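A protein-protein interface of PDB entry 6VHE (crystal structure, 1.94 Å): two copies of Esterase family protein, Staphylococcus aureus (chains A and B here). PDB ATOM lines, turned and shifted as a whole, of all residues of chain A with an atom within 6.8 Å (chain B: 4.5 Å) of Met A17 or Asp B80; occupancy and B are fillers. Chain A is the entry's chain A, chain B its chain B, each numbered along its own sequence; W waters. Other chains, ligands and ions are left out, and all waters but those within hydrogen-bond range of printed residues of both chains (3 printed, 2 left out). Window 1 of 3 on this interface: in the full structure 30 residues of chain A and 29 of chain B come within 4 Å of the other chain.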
ATOM      1  N   ASN A   9     -11.272 -12.290 -18.010  1.00  0.00           N
ATOM      2  CA  ASN A   9     -11.817 -11.111 -18.676  1.00  0.00           C
ATOM      3  C   ASN A   9     -12.852 -10.493 -17.751  1.00  0.00           C
ATOM      4  O   ASN A   9     -13.888 -11.110 -17.462  1.00  0.00           O
ATOM      5  CB  ASN A   9     -12.419 -11.466 -20.032  1.00  0.00           C
ATOM      6  CG  ASN A   9     -12.920 -10.241 -20.772  1.00  0.00           C
ATOM      7  OD1 ASN A   9     -13.710  -9.460 -20.233  1.00  0.00           O
ATOM      8  ND2 ASN A   9     -12.448 -10.054 -22.002  1.00  0.00           N
ATOM      9  N   TYR A  10     -12.573  -9.283 -17.275  1.00  0.00           N
ATOM     10  CA  TYR A  10     -13.485  -8.598 -16.372  1.00  0.00           C
ATOM     11  C   TYR A  10     -13.659  -7.150 -16.816  1.00  0.00           C
ATOM     12  O   TYR A  10     -12.802  -6.584 -17.507  1.00  0.00           O
ATOM     13  CB  TYR A  10     -13.002  -8.690 -14.902  1.00  0.00           C
ATOM     14  CG  TYR A  10     -11.821  -7.815 -14.515  1.00  0.00           C
ATOM     15  CD1 TYR A  10     -10.520  -8.283 -14.579  1.00  0.00           C
ATOM     16  CD2 TYR A  10     -12.023  -6.528 -14.064  1.00  0.00           C
ATOM     17  CE1 TYR A  10      -9.450  -7.473 -14.211  1.00  0.00           C
ATOM     18  CE2 TYR A  10     -10.969  -5.710 -13.703  1.00  0.00           C
ATOM     19  CZ  TYR A  10      -9.688  -6.180 -13.768  1.00  0.00           C
ATOM     20  OH  TYR A  10      -8.656  -5.334 -13.389  1.00  0.00           O
ATOM     21  N   HIS A  11     -14.794  -6.567 -16.428  1.00  0.00           N
ATOM     22  CA  HIS A  11     -15.052  -5.161 -16.695  1.00  0.00           C
ATOM     23  C   HIS A  11     -14.292  -4.311 -15.688  1.00  0.00           C
ATOM     24  O   HIS A  11     -14.589  -4.349 -14.488  1.00  0.00           O
ATOM     25  CB  HIS A  11     -16.541  -4.844 -16.620  1.00  0.00           C
ATOM     26  CG  HIS A  11     -16.864  -3.467 -17.102  1.00  0.00           C
ATOM     27  ND1 HIS A  11     -16.471  -2.335 -16.423  1.00  0.00           N
ATOM     28  CD2 HIS A  11     -17.494  -3.035 -18.218  1.00  0.00           C
ATOM     29  CE1 HIS A  11     -16.856  -1.265 -17.092  1.00  0.00           C
ATOM     30  NE2 HIS A  11     -17.480  -1.662 -18.186  1.00  0.00           N
ATOM     31  N   SER A  12     -13.341  -3.527 -16.181  1.00  0.00           N
ATOM     32  CA  SER A  12     -12.478  -2.718 -15.329  1.00  0.00           C
ATOM     33  C   SER A  12     -13.143  -1.391 -15.008  1.00  0.00           C
ATOM     34  O   SER A  12     -13.438  -0.623 -15.931  1.00  0.00           O
ATOM     35  CB  SER A  12     -11.158  -2.446 -16.001  1.00  0.00           C
ATOM     36  OG  SER A  12     -10.381  -1.553 -15.191  1.00  0.00           O
ATOM     37  N   PRO A  13     -13.360  -1.062 -13.742  1.00  0.00           N
ATOM     38  CA  PRO A  13     -13.854   0.281 -13.432  1.00  0.00           C
ATOM     39  C   PRO A  13     -12.869   1.370 -13.823  1.00  0.00           C
ATOM     40  O   PRO A  13     -13.296   2.481 -14.147  1.00  0.00           O
ATOM     41  CB  PRO A  13     -14.098   0.229 -11.911  1.00  0.00           C
ATOM     42  CG  PRO A  13     -13.361  -0.952 -11.422  1.00  0.00           C
ATOM     43  CD  PRO A  13     -13.302  -1.929 -12.553  1.00  0.00           C
ATOM     44  N   THR A  14     -11.567   1.071 -13.843  1.00  0.00           N
ATOM     45  CA  THR A  14     -10.569   2.091 -14.148  1.00  0.00           C
ATOM     46  C   THR A  14     -10.562   2.446 -15.633  1.00  0.00           C
ATOM     47  O   THR A  14     -10.538   3.627 -15.987  1.00  0.00           O
ATOM     48  CB  THR A  14      -9.173   1.641 -13.686  1.00  0.00           C
ATOM     49  OG1 THR A  14      -9.174   1.452 -12.263  1.00  0.00           O
ATOM     50  CG2 THR A  14      -8.130   2.716 -14.028  1.00  0.00           C
ATOM     51  N   ILE A  15     -10.585   1.459 -16.532  1.00  0.00           N
ATOM     52  CA  ILE A  15     -10.495   1.808 -17.954  1.00  0.00           C
ATOM     53  C   ILE A  15     -11.841   1.719 -18.672  1.00  0.00           C
ATOM     54  O   ILE A  15     -11.901   1.930 -19.886  1.00  0.00           O
ATOM     55  CB  ILE A  15      -9.419   0.987 -18.681  1.00  0.00           C
ATOM     56  CG1 ILE A  15      -9.676  -0.517 -18.538  1.00  0.00           C
ATOM     57  CG2 ILE A  15      -8.033   1.348 -18.141  1.00  0.00           C
ATOM     58  CD1 ILE A  15      -8.605  -1.349 -19.247  1.00  0.00           C
ATOM     59  N   GLY A  16     -12.926   1.457 -17.946  1.00  0.00           N
ATOM     60  CA  GLY A  16     -14.257   1.526 -18.523  1.00  0.00           C
ATOM     61  C   GLY A  16     -14.562   0.497 -19.592  1.00  0.00           C
ATOM     62  O   GLY A  16     -15.337   0.782 -20.509  1.00  0.00           O
ATOM     63  N   MET A  17     -13.999  -0.700 -19.497  1.00  0.00           N
ATOM     64  CA  MET A  17     -14.315  -1.713 -20.497  1.00  0.00           C
ATOM     65  C   MET A  17     -13.897  -3.080 -19.983  1.00  0.00           C
ATOM     66  O   MET A  17     -13.062  -3.203 -19.079  1.00  0.00           O
ATOM     67  CB  MET A  17     -13.618  -1.420 -21.838  1.00  0.00           C
ATOM     68  CG  MET A  17     -12.110  -1.450 -21.739  1.00  0.00           C
ATOM     69  SD  MET A  17     -11.296  -1.019 -23.290  1.00  0.00           S
ATOM     70  CE  MET A  17      -9.609  -0.871 -22.714  1.00  0.00           C
ATOM     71  N   HIS A  18     -14.487  -4.114 -20.581  1.00  0.00           N
ATOM     72  CA  HIS A  18     -13.933  -5.453 -20.437  1.00  0.00           C
ATOM     73  C   HIS A  18     -12.539  -5.497 -21.047  1.00  0.00           C
ATOM     74  O   HIS A  18     -12.272  -4.870 -22.075  1.00  0.00           O
ATOM     75  CB  HIS A  18     -14.834  -6.489 -21.118  1.00  0.00           C
ATOM     76  CG  HIS A  18     -16.124  -6.719 -20.402  1.00  0.00           C
ATOM     77  ND1 HIS A  18     -17.183  -5.835 -20.464  1.00  0.00           N
ATOM     78  CD2 HIS A  18     -16.515  -7.723 -19.587  1.00  0.00           C
ATOM     79  CE1 HIS A  18     -18.182  -6.301 -19.732  1.00  0.00           C
ATOM     80  NE2 HIS A  18     -17.797  -7.439 -19.183  1.00  0.00           N
ATOM     81  N   GLN A  19     -11.654  -6.258 -20.410  1.00  0.00           N
ATOM     82  CA  GLN A  19     -10.268  -6.390 -20.816  1.00  0.00           C
ATOM     83  C   GLN A  19      -9.784  -7.772 -20.405  1.00  0.00           C
ATOM     84  O   GLN A  19     -10.149  -8.249 -19.332  1.00  0.00           O
ATOM     85  CB  GLN A  19      -9.402  -5.316 -20.150  1.00  0.00           C
ATOM     86  CG  GLN A  19      -7.999  -5.194 -20.757  1.00  0.00           C
ATOM     87  CD  GLN A  19      -7.940  -4.225 -21.939  1.00  0.00           C
ATOM     88  OE1 GLN A  19      -8.921  -4.048 -22.669  1.00  0.00           O
ATOM     89  NE2 GLN A  19      -6.780  -3.601 -22.134  1.00  0.00           N
ATOM     90  N   ASN A  78      -2.887  -6.387 -20.336  1.00  0.00           N
ATOM     91  CA  ASN A  78      -2.853  -5.812 -21.674  1.00  0.00           C
ATOM     92  C   ASN A  78      -3.031  -4.306 -21.564  1.00  0.00           C
ATOM     93  O   ASN A  78      -3.998  -3.840 -20.947  1.00  0.00           O
ATOM     94  CB  ASN A  78      -3.961  -6.406 -22.550  1.00  0.00           C
ATOM     95  CG  ASN A  78      -4.043  -5.725 -23.921  1.00  0.00           C
ATOM     96  OD1 ASN A  78      -3.028  -5.337 -24.492  1.00  0.00           O
ATOM     97  ND2 ASN A  78      -5.251  -5.564 -24.434  1.00  0.00           N
ATOM     98  N   ASP A  80      -2.172  -2.293 -24.551  1.00  0.00           N
ATOM     99  CA  ASP A  80      -2.331  -1.716 -25.890  1.00  0.00           C
ATOM    100  C   ASP A  80      -1.094  -0.904 -26.300  1.00  0.00           C
ATOM    101  O   ASP A  80       0.038  -1.353 -26.095  1.00  0.00           O
ATOM    102  CB  ASP A  80      -3.608  -0.857 -25.886  1.00  0.00           C
ATOM    103  CG  ASP A  80      -4.260  -0.732 -27.249  1.00  0.00           C
ATOM    104  OD1 ASP A  80      -5.153  -1.551 -27.557  1.00  0.00           O
ATOM    105  OD2 ASP A  80      -3.907   0.213 -27.992  1.00  0.00           O
ATOM    106  N   HIS A  91      -6.886   5.777 -22.463  1.00  0.00           N
ATOM    107  CA  HIS A  91      -7.263   5.122 -21.216  1.00  0.00           C
ATOM    108  C   HIS A  91      -6.272   5.432 -20.099  1.00  0.00           C
ATOM    109  O   HIS A  91      -5.104   5.754 -20.344  1.00  0.00           O
ATOM    110  CB  HIS A  91      -7.349   3.598 -21.396  1.00  0.00           C
ATOM    111  CG  HIS A  91      -8.464   3.160 -22.290  1.00  0.00           C
ATOM    112  ND1 HIS A  91      -9.757   3.002 -21.840  1.00  0.00           N
ATOM    113  CD2 HIS A  91      -8.485   2.863 -23.613  1.00  0.00           C
ATOM    114  CE1 HIS A  91     -10.524   2.605 -22.842  1.00  0.00           C
ATOM    115  NE2 HIS A  91      -9.777   2.516 -23.930  1.00  0.00           N
ATOM    116  N   TYR A  93      -4.170   3.913 -18.212  1.00  0.00           N
ATOM    117  CA  TYR A  93      -3.485   2.632 -18.147  1.00  0.00           C
ATOM    118  C   TYR A  93      -2.429   2.546 -17.044  1.00  0.00           C
ATOM    119  O   TYR A  93      -2.070   1.436 -16.639  1.00  0.00           O
ATOM    120  CB  TYR A  93      -2.869   2.310 -19.509  1.00  0.00           C
ATOM    121  CG  TYR A  93      -3.798   1.534 -20.424  1.00  0.00           C
ATOM    122  CD1 TYR A  93      -4.298   0.280 -20.051  1.00  0.00           C
ATOM    123  CD2 TYR A  93      -4.176   2.049 -21.663  1.00  0.00           C
ATOM    124  CE1 TYR A  93      -5.140  -0.423 -20.893  1.00  0.00           C
ATOM    125  CE2 TYR A  93      -4.997   1.338 -22.519  1.00  0.00           C
ATOM    126  CZ  TYR A  93      -5.478   0.109 -22.127  1.00  0.00           C
ATOM    127  OH  TYR A  93      -6.297  -0.591 -22.978  1.00  0.00           O
ATOM    128  N   TYR A  96      -4.532   1.566 -14.324  1.00  0.00           N
ATOM    129  CA  TYR A  96      -5.022   0.211 -14.587  1.00  0.00           C
ATOM    130  C   TYR A  96      -4.074  -0.845 -14.031  1.00  0.00           C
ATOM    131  O   TYR A  96      -4.517  -1.845 -13.460  1.00  0.00           O
ATOM    132  CB  TYR A  96      -5.221   0.000 -16.095  1.00  0.00           C
ATOM    133  CG  TYR A  96      -5.731  -1.389 -16.447  1.00  0.00           C
ATOM    134  CD1 TYR A  96      -6.963  -1.841 -15.978  1.00  0.00           C
ATOM    135  CD2 TYR A  96      -4.989  -2.239 -17.253  1.00  0.00           C
ATOM    136  CE1 TYR A  96      -7.427  -3.125 -16.290  1.00  0.00           C
ATOM    137  CE2 TYR A  96      -5.450  -3.507 -17.574  1.00  0.00           C
ATOM    138  CZ  TYR A  96      -6.669  -3.941 -17.087  1.00  0.00           C
ATOM    139  OH  TYR A  96      -7.134  -5.194 -17.411  1.00  0.00           O
ATOM    140  N   HIS B  48     -19.691  -4.840 -30.986  1.00  0.00           N
ATOM    141  CA  HIS B  48     -20.042  -4.575 -29.595  1.00  0.00           C
ATOM    142  C   HIS B  48     -20.248  -3.080 -29.346  1.00  0.00           C
ATOM    143  O   HIS B  48     -19.817  -2.223 -30.121  1.00  0.00           O
ATOM    144  CB  HIS B  48     -18.953  -5.121 -28.675  1.00  0.00           C
ATOM    145  CG  HIS B  48     -17.627  -4.446 -28.848  1.00  0.00           C
ATOM    146  ND1 HIS B  48     -17.341  -3.224 -28.283  1.00  0.00           N
ATOM    147  CD2 HIS B  48     -16.506  -4.828 -29.509  1.00  0.00           C
ATOM    148  CE1 HIS B  48     -16.102  -2.877 -28.592  1.00  0.00           C
ATOM    149  NE2 HIS B  48     -15.576  -3.831 -29.341  1.00  0.00           N
ATOM    150  N   SER B  51     -17.779  -0.303 -23.830  1.00  0.00           N
ATOM    151  CA  SER B  51     -17.364  -1.031 -22.626  1.00  0.00           C
ATOM    152  C   SER B  51     -17.388  -2.535 -22.847  1.00  0.00           C
ATOM    153  O   SER B  51     -16.844  -3.271 -22.027  1.00  0.00           O
ATOM    154  CB  SER B  51     -18.177  -0.677 -21.365  1.00  0.00           C
ATOM    155  OG  SER B  51     -19.378  -1.421 -21.260  1.00  0.00           O
ATOM    156  N   ASN B  78     -13.019  -6.767 -31.559  1.00  0.00           N
ATOM    157  CA  ASN B  78     -12.857  -5.856 -30.426  1.00  0.00           C
ATOM    158  C   ASN B  78     -12.298  -4.530 -30.933  1.00  0.00           C
ATOM    159  O   ASN B  78     -11.231  -4.515 -31.563  1.00  0.00           O
ATOM    160  CB  ASN B  78     -11.916  -6.450 -29.368  1.00  0.00           C
ATOM    161  CG  ASN B  78     -11.613  -5.457 -28.231  1.00  0.00           C
ATOM    162  OD1 ASN B  78     -12.455  -4.618 -27.872  1.00  0.00           O
ATOM    163  ND2 ASN B  78     -10.404  -5.534 -27.685  1.00  0.00           N
ATOM    164  N   VAL B  79     -12.998  -3.421 -30.652  1.00  0.00           N
ATOM    165  CA  VAL B  79     -12.519  -2.110 -31.107  1.00  0.00           C
ATOM    166  C   VAL B  79     -12.435  -1.112 -29.958  1.00  0.00           C
ATOM    167  O   VAL B  79     -12.313   0.101 -30.197  1.00  0.00           O
ATOM    168  CB  VAL B  79     -13.392  -1.533 -32.247  1.00  0.00           C
ATOM    169  CG1 VAL B  79     -13.605  -2.558 -33.348  1.00  0.00           C
ATOM    170  CG2 VAL B  79     -14.726  -1.014 -31.713  1.00  0.00           C
ATOM    171  N   ASP B  80     -12.501  -1.596 -28.715  1.00  0.00           N
ATOM    172  CA  ASP B  80     -12.154  -0.753 -27.551  1.00  0.00           C
ATOM    173  C   ASP B  80     -13.135   0.420 -27.449  1.00  0.00           C
ATOM    174  O   ASP B  80     -14.357   0.209 -27.550  1.00  0.00           O
ATOM    175  CB  ASP B  80     -10.685  -0.373 -27.727  1.00  0.00           C
ATOM    176  CG  ASP B  80     -10.058   0.117 -26.458  1.00  0.00           C
ATOM    177  OD1 ASP B  80      -9.275  -0.650 -25.855  1.00  0.00           O
ATOM    178  OD2 ASP B  80     -10.344   1.265 -26.072  1.00  0.00           O
ATOM    179  N   HIS B  81     -12.662   1.660 -27.264  1.00  0.00           N
ATOM    180  CA  HIS B  81     -13.494   2.852 -27.112  1.00  0.00           C
ATOM    181  C   HIS B  81     -13.535   3.694 -28.389  1.00  0.00           C
ATOM    182  O   HIS B  81     -13.811   4.895 -28.327  1.00  0.00           O
ATOM    183  CB  HIS B  81     -12.979   3.706 -25.943  1.00  0.00           C
ATOM    184  CG  HIS B  81     -13.461   3.252 -24.595  1.00  0.00           C
ATOM    185  ND1 HIS B  81     -13.460   4.076 -23.489  1.00  0.00           N
ATOM    186  CD2 HIS B  81     -13.942   2.055 -24.171  1.00  0.00           C
ATOM    187  CE1 HIS B  81     -13.945   3.416 -22.447  1.00  0.00           C
ATOM    188  NE2 HIS B  81     -14.240   2.186 -22.832  1.00  0.00           N
ATOM    189  N   SER B  82     -13.274   3.081 -29.543  1.00  0.00           N
ATOM    190  CA  SER B  82     -12.940   3.815 -30.759  1.00  0.00           C
ATOM    191  C   SER B  82     -14.149   4.310 -31.539  1.00  0.00           C
ATOM    192  O   SER B  82     -13.963   5.060 -32.498  1.00  0.00           O
ATOM    193  CB  SER B  82     -12.114   2.932 -31.686  1.00  0.00           C
ATOM    194  OG  SER B  82     -12.932   1.898 -32.232  1.00  0.00           O
ATOM    195  N   TYR B  93      -9.291   1.944 -36.475  1.00  0.00           N
ATOM    196  CA  TYR B  93     -10.249   0.882 -36.189  1.00  0.00           C
ATOM    197  C   TYR B  93     -11.335   0.743 -37.251  1.00  0.00           C
ATOM    198  O   TYR B  93     -11.914  -0.342 -37.380  1.00  0.00           O
ATOM    199  CB  TYR B  93     -10.888   1.097 -34.818  1.00  0.00           C
ATOM    200  CG  TYR B  93     -10.167   0.401 -33.699  1.00  0.00           C
ATOM    201  CD1 TYR B  93     -10.022  -0.995 -33.685  1.00  0.00           C
ATOM    202  CD2 TYR B  93      -9.621   1.127 -32.644  1.00  0.00           C
ATOM    203  CE1 TYR B  93      -9.355  -1.630 -32.651  1.00  0.00           C
ATOM    204  CE2 TYR B  93      -8.980   0.488 -31.582  1.00  0.00           C
ATOM    205  CZ  TYR B  93      -8.846  -0.886 -31.603  1.00  0.00           C
ATOM    206  OH  TYR B  93      -8.202  -1.510 -30.568  1.00  0.00           O
ATOM    207  N   MET B 124     -22.893   1.810 -29.369  1.00  0.00           N
ATOM    208  CA  MET B 124     -21.743   2.172 -30.195  1.00  0.00           C
ATOM    209  C   MET B 124     -21.592   1.241 -31.399  1.00  0.00           C
ATOM    210  O   MET B 124     -21.126   1.668 -32.461  1.00  0.00           O
ATOM    211  CB  MET B 124     -20.470   2.169 -29.330  1.00  0.00           C
ATOM    212  CG  MET B 124     -19.191   2.676 -30.033  1.00  0.00           C
ATOM    213  SD  MET B 124     -17.674   2.476 -29.064  1.00  0.00           S
ATOM    214  CE  MET B 124     -17.404   0.698 -29.149  1.00  0.00           C
HETATM  215  O   HOH W   1     -13.048  -3.614 -25.442  1.00  0.00           O
HETATM  216  O   HOH W   2      -9.476  -3.463 -25.748  1.00  0.00           O
HETATM  217  O   HOH W   3      -7.390  -0.084 -28.607  1.00  0.00           O
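His A11 touches Ser B51. Ile A15 touches His B81. O of Gly A16 touches CB of Ser B51, at 3.3 Å. Met A17 touches Ser B51 (CA to O, 3.3 Å). CB of Met A17 touches NE2 of His B81 (3.8 Å). ND1 of His B81 touches CE1 of His A91, at 3.3 Å.
A ring nitrogen (NE2) of His B81 lies within hydrogen-bond range of the backbone carbonyl oxygen (O) of Gly A16. O of Ser B51 sits at hydrogen-bond distance from N of His A18 (2.9 Å). OD2 of Asp B80 is in hydrogen-bond range of NE2 of His A91, at 2.5 Å. The side-chain carboxylate of Asp B80 lies close to the side-chain sulfur of Met A17 (3.3 Å).
3 positions are printed for both chains. Of the 10 pairs that touch across the chains among the printed residues, none has its exchanged pair printed and touching as well.
Printed residues of chain B that touch a printed residue of chain A: Ser B51, Asp B80 and His B81. Hydrophobic or aromatic side chains of chain B that line the printed part of chain A: His B81. Of the 16 printed residues of chain A, 6 touch a printed residue of chain B. Hydrophobic or aromatic side chains of chain A that line the printed part of chain B: His A11, Met A17, His A18 and His A91.
The backbone NH (N) of Ile A15 sits at hydrogen-bond distance from the side-chain hydroxyl (OG) of Ser A12, at 3.3 Å. O of Met A17 is in hydrogen-bond range of N of Ser A12 (2.9 Å). ND1 of His A91 lies within hydrogen-bond range of O of Ile A15, 3.1 Å away. The side-chain amide oxygen (OD1) of Asn B78 lies within hydrogen-bond range of the backbone NH (N) of Asp B80 (3.1 Å).
Water W3 lies within hydrogen-bond range of OH of Tyr B93, OD1 of Asp A80 and OD1 of Asp B80. Water W1 bridges the side-chain amide oxygen of Asn B78 (2.7 Å) and the side-chain sulfur of Met A17 (3.8 Å). Water W2 lies within hydrogen-bond range of the side-chain carboxylate (OD1) of Asp B80 (2.8 Å), the side-chain amide nitrogen (ND2) of Asn B78 (3.0 Å) and the side-chain amide oxygen (OE1) of Gln A19 (3.2 Å).
Printed residues of chain B within 4 Å of His A18: Ser B51. Of the printed residues of chain B, His A91 touches Asp B80 and His B81. Tyr A96 touches none of the printed residues of chain B. Of chain A, only Met A17 (3.2 Å) and His A91 (2.5 Å) come within 4 Å of Asp B80. The nearest residue of chain A that does not touch Asp B80 is Tyr A93 (4.1 Å). The nearest printed residue of chain B that does not touch His A91 is Ser B82 (6.6 Å).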
